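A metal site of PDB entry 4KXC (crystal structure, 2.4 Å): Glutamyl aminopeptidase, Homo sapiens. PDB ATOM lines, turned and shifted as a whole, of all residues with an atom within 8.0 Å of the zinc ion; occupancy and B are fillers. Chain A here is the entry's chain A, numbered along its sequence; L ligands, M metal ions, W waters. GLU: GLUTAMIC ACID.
Water W1 lies within hydrogen-bond range of a nitrogen (N) of the ligand, the side-chain carboxylate of Glu 319 and the side-chain carboxylate of Glu 285.
The zinc ion is bound by the side-chain carboxylate of Glu 341 (2.0 Å), a ring nitrogen (NE2) of His 322 (2.1 Å) and a ring nitrogen (NE2) of His 318 (2.1 Å). The zinc ion has three donor atoms within binding distance. Slightly farther from the zinc ion lies water W1 (2.7 Å).
OH of Tyr 404 touches the zinc ion (3.96 Å). The nearest printed residue that does not touch the zinc ion is Ala 344 (4.2 Å).
An oxygen (O) of the ligand sits close to the backbone carbonyl oxygen (O) of Ala 283 (3.0 Å). OE1 of Glu 285 is in salt-bridge range of N of the ligand. A nitrogen (N) of the ligand is in salt-bridge range of the side-chain carboxylate (OE2) of Glu 341 (3.2 Å). The side-chain hydroxyl (OH) of Tyr 404 is in hydrogen-bond range of an oxygen (OXT) of the ligand (2.5 Å). The side-chain carboxylate of Glu 148 lies within salt-bridge range of a nitrogen (N) of the ligand, 3.6 Å away.
ND1 of His 318 is in hydrogen-bond range of OE2 of Glu 348. A ring nitrogen (ND1) of His 318 lies within hydrogen-bond range of the backbone carbonyl oxygen (O) of Ala 344 (3.5 Å). ND1 of His 322 is in hydrogen-bond range of O of Phe 325 (3.0 Å). The side-chain carboxylate (OE1) of Glu 341 sits close to the side-chain hydroxyl (OH) of Tyr 404. The backbone carbonyl oxygen (O) of Glu 341 is in hydrogen-bond range of the side-chain hydroxyl (OG) of Ser 345. A ring nitrogen (ND1) of His 322 is in hydrogen-bond range of the side-chain carboxylate (OE2) of Glu 285, 3.4 Å away.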
ATOM      1  N   GLU A 148      17.650  28.274 -18.166  1.00  0.00           N
ATOM      2  CA  GLU A 148      18.686  27.265 -18.375  1.00  0.00           C
ATOM      3  C   GLU A 148      18.210  25.862 -18.020  1.00  0.00           C
ATOM      4  O   GLU A 148      17.758  25.632 -16.893  1.00  0.00           O
ATOM      5  CB  GLU A 148      19.967  27.605 -17.597  1.00  0.00           C
ATOM      6  CG  GLU A 148      21.198  26.903 -18.153  1.00  0.00           C
ATOM      7  CD  GLU A 148      22.488  27.372 -17.507  1.00  0.00           C
ATOM      8  OE1 GLU A 148      22.455  27.842 -16.344  1.00  0.00           O
ATOM      9  OE2 GLU A 148      23.529  27.266 -18.183  1.00  0.00           O
ATOM     10  N   ALA A 283      20.299  29.553  -8.171  1.00  0.00           N
ATOM     11  CA  ALA A 283      20.579  30.879  -8.692  1.00  0.00           C
ATOM     12  C   ALA A 283      20.876  30.726 -10.182  1.00  0.00           C
ATOM     13  O   ALA A 283      21.208  29.630 -10.641  1.00  0.00           O
ATOM     14  CB  ALA A 283      21.769  31.503  -7.982  1.00  0.00           C
ATOM     15  N   MET A 284      20.761  31.827 -10.921  1.00  0.00           N
ATOM     16  CA  MET A 284      20.896  31.811 -12.376  1.00  0.00           C
ATOM     17  C   MET A 284      21.600  33.077 -12.871  1.00  0.00           C
ATOM     18  O   MET A 284      21.185  34.188 -12.565  1.00  0.00           O
ATOM     19  CB  MET A 284      19.513  31.657 -13.026  1.00  0.00           C
ATOM     20  CG  MET A 284      19.574  31.461 -14.528  1.00  0.00           C
ATOM     21  SD  MET A 284      20.926  30.359 -14.994  1.00  0.00           S
ATOM     22  CE  MET A 284      21.109  30.812 -16.712  1.00  0.00           C
ATOM     23  N   GLU A 285      22.658  32.880 -13.657  1.00  0.00           N
ATOM     24  CA  GLU A 285      23.612  33.944 -14.018  1.00  0.00           C
ATOM     25  C   GLU A 285      23.221  34.860 -15.177  1.00  0.00           C
ATOM     26  O   GLU A 285      24.090  35.376 -15.899  1.00  0.00           O
ATOM     27  CB  GLU A 285      24.973  33.321 -14.339  1.00  0.00           C
ATOM     28  CG  GLU A 285      24.976  32.479 -15.616  1.00  0.00           C
ATOM     29  CD  GLU A 285      24.752  31.000 -15.369  1.00  0.00           C
ATOM     30  OE1 GLU A 285      24.005  30.633 -14.429  1.00  0.00           O
ATOM     31  OE2 GLU A 285      25.333  30.202 -16.127  1.00  0.00           O
ATOM     32  N   VAL A 315      27.713  31.317  -3.576  1.00  0.00           N
ATOM     33  CA  VAL A 315      26.795  31.372  -4.714  1.00  0.00           C
ATOM     34  C   VAL A 315      26.915  32.716  -5.437  1.00  0.00           C
ATOM     35  O   VAL A 315      26.982  32.763  -6.659  1.00  0.00           O
ATOM     36  CB  VAL A 315      25.332  31.086  -4.318  1.00  0.00           C
ATOM     37  CG1 VAL A 315      24.441  31.149  -5.546  1.00  0.00           C
ATOM     38  CG2 VAL A 315      25.214  29.720  -3.655  1.00  0.00           C
ATOM     39  N   HIS A 318      30.093  32.515  -7.291  1.00  0.00           N
ATOM     40  CA  HIS A 318      29.810  31.601  -8.395  1.00  0.00           C
ATOM     41  C   HIS A 318      29.113  32.333  -9.539  1.00  0.00           C
ATOM     42  O   HIS A 318      29.533  32.246 -10.694  1.00  0.00           O
ATOM     43  CB  HIS A 318      28.926  30.454  -7.899  1.00  0.00           C
ATOM     44  CG  HIS A 318      28.719  29.351  -8.901  1.00  0.00           C
ATOM     45  ND1 HIS A 318      29.487  28.211  -8.921  1.00  0.00           N
ATOM     46  CD2 HIS A 318      27.830  29.225  -9.915  1.00  0.00           C
ATOM     47  CE1 HIS A 318      29.081  27.425  -9.907  1.00  0.00           C
ATOM     48  NE2 HIS A 318      28.075  28.018 -10.524  1.00  0.00           N
ATOM     49  N   GLU A 319      28.034  33.060  -9.212  1.00  0.00           N
ATOM     50  CA  GLU A 319      27.210  33.719 -10.213  1.00  0.00           C
ATOM     51  C   GLU A 319      27.987  34.806 -10.939  1.00  0.00           C
ATOM     52  O   GLU A 319      27.764  35.072 -12.124  1.00  0.00           O
ATOM     53  CB  GLU A 319      25.953  34.308  -9.570  1.00  0.00           C
ATOM     54  CG  GLU A 319      25.032  33.278  -8.915  1.00  0.00           C
ATOM     55  CD  GLU A 319      24.779  32.075  -9.801  1.00  0.00           C
ATOM     56  OE1 GLU A 319      24.481  32.255 -10.995  1.00  0.00           O
ATOM     57  OE2 GLU A 319      24.861  30.936  -9.281  1.00  0.00           O
ATOM     58  N   VAL A 321      31.352  34.702 -11.429  1.00  0.00           N
ATOM     59  CA  VAL A 321      32.310  34.053 -12.327  1.00  0.00           C
ATOM     60  C   VAL A 321      31.674  33.871 -13.693  1.00  0.00           C
ATOM     61  O   VAL A 321      32.328  34.055 -14.731  1.00  0.00           O
ATOM     62  CB  VAL A 321      32.802  32.682 -11.803  1.00  0.00           C
ATOM     63  CG1 VAL A 321      33.799  32.079 -12.783  1.00  0.00           C
ATOM     64  CG2 VAL A 321      33.453  32.812 -10.442  1.00  0.00           C
ATOM     65  N   HIS A 322      30.390  33.549 -13.693  1.00  0.00           N
ATOM     66  CA  HIS A 322      29.671  33.283 -14.924  1.00  0.00           C
ATOM     67  C   HIS A 322      29.618  34.464 -15.874  1.00  0.00           C
ATOM     68  O   HIS A 322      29.489  34.286 -17.081  1.00  0.00           O
ATOM     69  CB  HIS A 322      28.266  32.786 -14.636  1.00  0.00           C
ATOM     70  CG  HIS A 322      28.181  31.308 -14.392  1.00  0.00           C
ATOM     71  ND1 HIS A 322      28.640  30.375 -15.286  1.00  0.00           N
ATOM     72  CD2 HIS A 322      27.659  30.614 -13.350  1.00  0.00           C
ATOM     73  CE1 HIS A 322      28.413  29.165 -14.806  1.00  0.00           C
ATOM     74  NE2 HIS A 322      27.820  29.282 -13.639  1.00  0.00           N
ATOM     75  N   PHE A 325      33.039  33.485 -17.463  1.00  0.00           N
ATOM     76  CA  PHE A 325      32.988  32.082 -17.904  1.00  0.00           C
ATOM     77  C   PHE A 325      31.564  31.568 -17.963  1.00  0.00           C
ATOM     78  O   PHE A 325      30.986  31.163 -16.948  1.00  0.00           O
ATOM     79  CB  PHE A 325      33.864  31.206 -17.023  1.00  0.00           C
ATOM     80  CG  PHE A 325      35.323  31.413 -17.247  1.00  0.00           C
ATOM     81  CD1 PHE A 325      35.969  30.789 -18.306  1.00  0.00           C
ATOM     82  CD2 PHE A 325      36.061  32.251 -16.420  1.00  0.00           C
ATOM     83  CE1 PHE A 325      37.320  30.994 -18.535  1.00  0.00           C
ATOM     84  CE2 PHE A 325      37.403  32.455 -16.643  1.00  0.00           C
ATOM     85  CZ  PHE A 325      38.039  31.821 -17.701  1.00  0.00           C
ATOM     86  N   LEU A 337      29.477  21.625 -21.009  1.00  0.00           N
ATOM     87  CA  LEU A 337      28.876  22.430 -19.932  1.00  0.00           C
ATOM     88  C   LEU A 337      29.865  22.755 -18.805  1.00  0.00           C
ATOM     89  O   LEU A 337      29.769  23.824 -18.196  1.00  0.00           O
ATOM     90  CB  LEU A 337      27.640  21.754 -19.347  1.00  0.00           C
ATOM     91  CG  LEU A 337      26.996  22.390 -18.107  1.00  0.00           C
ATOM     92  CD1 LEU A 337      26.351  23.729 -18.442  1.00  0.00           C
ATOM     93  CD2 LEU A 337      25.984  21.442 -17.486  1.00  0.00           C
ATOM     94  N   ASN A 340      31.460  26.095 -18.367  1.00  0.00           N
ATOM     95  CA  ASN A 340      30.703  27.068 -17.588  1.00  0.00           C
ATOM     96  C   ASN A 340      30.765  26.720 -16.103  1.00  0.00           C
ATOM     97  O   ASN A 340      31.291  27.493 -15.289  1.00  0.00           O
ATOM     98  CB  ASN A 340      29.235  27.117 -18.040  1.00  0.00           C
ATOM     99  CG  ASN A 340      29.029  27.916 -19.329  1.00  0.00           C
ATOM    100  OD1 ASN A 340      27.936  28.412 -19.586  1.00  0.00           O
ATOM    101  ND2 ASN A 340      30.078  28.025 -20.139  1.00  0.00           N
ATOM    102  N   GLU A 341      30.256  25.543 -15.752  1.00  0.00           N
ATOM    103  CA  GLU A 341      30.007  25.184 -14.356  1.00  0.00           C
ATOM    104  C   GLU A 341      31.240  24.817 -13.547  1.00  0.00           C
ATOM    105  O   GLU A 341      31.331  25.155 -12.366  1.00  0.00           O
ATOM    106  CB  GLU A 341      28.956  24.072 -14.265  1.00  0.00           C
ATOM    107  CG  GLU A 341      27.590  24.478 -14.819  1.00  0.00           C
ATOM    108  CD  GLU A 341      27.066  25.779 -14.241  1.00  0.00           C
ATOM    109  OE1 GLU A 341      27.402  26.144 -13.097  1.00  0.00           O
ATOM    110  OE2 GLU A 341      26.304  26.463 -14.958  1.00  0.00           O
ATOM    111  N   GLY A 342      32.169  24.115 -14.194  1.00  0.00           N
ATOM    112  CA  GLY A 342      33.437  23.778 -13.573  1.00  0.00           C
ATOM    113  C   GLY A 342      34.246  25.037 -13.271  1.00  0.00           C
ATOM    114  O   GLY A 342      34.828  25.160 -12.182  1.00  0.00           O
ATOM    115  N   PHE A 343      34.260  25.960 -14.228  1.00  0.00           N
ATOM    116  CA  PHE A 343      35.011  27.203 -14.083  1.00  0.00           C
ATOM    117  C   PHE A 343      34.438  28.057 -12.968  1.00  0.00           C
ATOM    118  O   PHE A 343      35.187  28.576 -12.136  1.00  0.00           O
ATOM    119  CB  PHE A 343      35.053  27.963 -15.400  1.00  0.00           C
ATOM    120  CG  PHE A 343      36.053  27.408 -16.363  1.00  0.00           C
ATOM    121  CD1 PHE A 343      35.875  26.135 -16.909  1.00  0.00           C
ATOM    122  CD2 PHE A 343      37.176  28.138 -16.714  1.00  0.00           C
ATOM    123  CE1 PHE A 343      36.799  25.622 -17.794  1.00  0.00           C
ATOM    124  CE2 PHE A 343      38.099  27.615 -17.602  1.00  0.00           C
ATOM    125  CZ  PHE A 343      37.914  26.360 -18.137  1.00  0.00           C
ATOM    126  N   ALA A 344      33.117  28.167 -12.950  1.00  0.00           N
ATOM    127  CA  ALA A 344      32.417  28.877 -11.884  1.00  0.00           C
ATOM    128  C   ALA A 344      32.601  28.174 -10.530  1.00  0.00           C
ATOM    129  O   ALA A 344      32.831  28.844  -9.511  1.00  0.00           O
ATOM    130  CB  ALA A 344      30.952  29.047 -12.226  1.00  0.00           C
ATOM    131  N   SER A 345      32.536  26.843 -10.531  1.00  0.00           N
ATOM    132  CA  SER A 345      32.759  26.074  -9.304  1.00  0.00           C
ATOM    133  C   SER A 345      34.212  26.173  -8.785  1.00  0.00           C
ATOM    134  O   SER A 345      34.441  26.027  -7.582  1.00  0.00           O
ATOM    135  CB  SER A 345      32.330  24.604  -9.473  1.00  0.00           C
ATOM    136  OG  SER A 345      30.916  24.493  -9.657  1.00  0.00           O
ATOM    137  N   GLU A 348      34.829  30.345  -7.730  1.00  0.00           N
ATOM    138  CA  GLU A 348      34.014  30.798  -6.601  1.00  0.00           C
ATOM    139  C   GLU A 348      34.844  30.845  -5.314  1.00  0.00           C
ATOM    140  O   GLU A 348      34.746  31.810  -4.556  1.00  0.00           O
ATOM    141  CB  GLU A 348      32.751  29.940  -6.434  1.00  0.00           C
ATOM    142  CG  GLU A 348      33.003  28.500  -6.032  1.00  0.00           C
ATOM    143  CD  GLU A 348      31.731  27.676  -5.871  1.00  0.00           C
ATOM    144  OE1 GLU A 348      31.763  26.699  -5.104  1.00  0.00           O
ATOM    145  OE2 GLU A 348      30.709  27.988  -6.500  1.00  0.00           O
ATOM    146  N   PHE A 399      23.733  18.831 -15.418  1.00  0.00           N
ATOM    147  CA  PHE A 399      23.950  19.821 -14.366  1.00  0.00           C
ATOM    148  C   PHE A 399      24.111  19.066 -13.043  1.00  0.00           C
ATOM    149  O   PHE A 399      23.182  19.022 -12.235  1.00  0.00           O
ATOM    150  CB  PHE A 399      22.786  20.803 -14.299  1.00  0.00           C
ATOM    151  CG  PHE A 399      22.771  21.797 -15.423  1.00  0.00           C
ATOM    152  CD1 PHE A 399      22.203  21.467 -16.652  1.00  0.00           C
ATOM    153  CD2 PHE A 399      23.332  23.057 -15.259  1.00  0.00           C
ATOM    154  CE1 PHE A 399      22.205  22.372 -17.709  1.00  0.00           C
ATOM    155  CE2 PHE A 399      23.339  23.960 -16.308  1.00  0.00           C
ATOM    156  CZ  PHE A 399      22.768  23.626 -17.525  1.00  0.00           C
ATOM    157  N   TYR A 404      30.142  20.151 -12.276  1.00  0.00           N
ATOM    158  CA  TYR A 404      30.504  21.132 -11.260  1.00  0.00           C
ATOM    159  C   TYR A 404      31.763  20.744 -10.489  1.00  0.00           C
ATOM    160  O   TYR A 404      32.792  21.418 -10.599  1.00  0.00           O
ATOM    161  CB  TYR A 404      29.342  21.350 -10.271  1.00  0.00           C
ATOM    162  CG  TYR A 404      28.185  22.179 -10.772  1.00  0.00           C
ATOM    163  CD1 TYR A 404      27.310  21.697 -11.746  1.00  0.00           C
ATOM    164  CD2 TYR A 404      27.943  23.444 -10.242  1.00  0.00           C
ATOM    165  CE1 TYR A 404      26.241  22.458 -12.193  1.00  0.00           C
ATOM    166  CE2 TYR A 404      26.867  24.214 -10.681  1.00  0.00           C
ATOM    167  CZ  TYR A 404      26.027  23.720 -11.658  1.00  0.00           C
ATOM    168  OH  TYR A 404      24.972  24.479 -12.102  1.00  0.00           O
HETATM  169  N   GLU L   1      23.943  27.601 -13.097  1.00  0.00           N
HETATM  170  CA  GLU L   1      22.958  27.454 -11.978  1.00  0.00           C
HETATM  171  C   GLU L   1      23.653  27.214 -10.627  1.00  0.00           C
HETATM  172  O   GLU L   1      23.654  28.076  -9.748  1.00  0.00           O
HETATM  173  CB  GLU L   1      21.925  26.370 -12.278  1.00  0.00           C
HETATM  174  CG  GLU L   1      21.008  26.692 -13.451  1.00  0.00           C
HETATM  175  CD  GLU L   1      19.876  25.708 -13.621  1.00  0.00           C
HETATM  176  OE1 GLU L   1      20.095  24.493 -13.436  1.00  0.00           O
HETATM  177  OE2 GLU L   1      18.742  26.142 -13.940  1.00  0.00           O
HETATM  178  OXT GLU L   1      24.231  26.153 -10.378  1.00  0.00           O
HETATM  179 ZN    ZN M   1      26.965  27.898 -12.311  1.00  0.00          ZN
HETATM  180  O   HOH W   1      24.946  29.633 -11.851  1.00  0.00           O
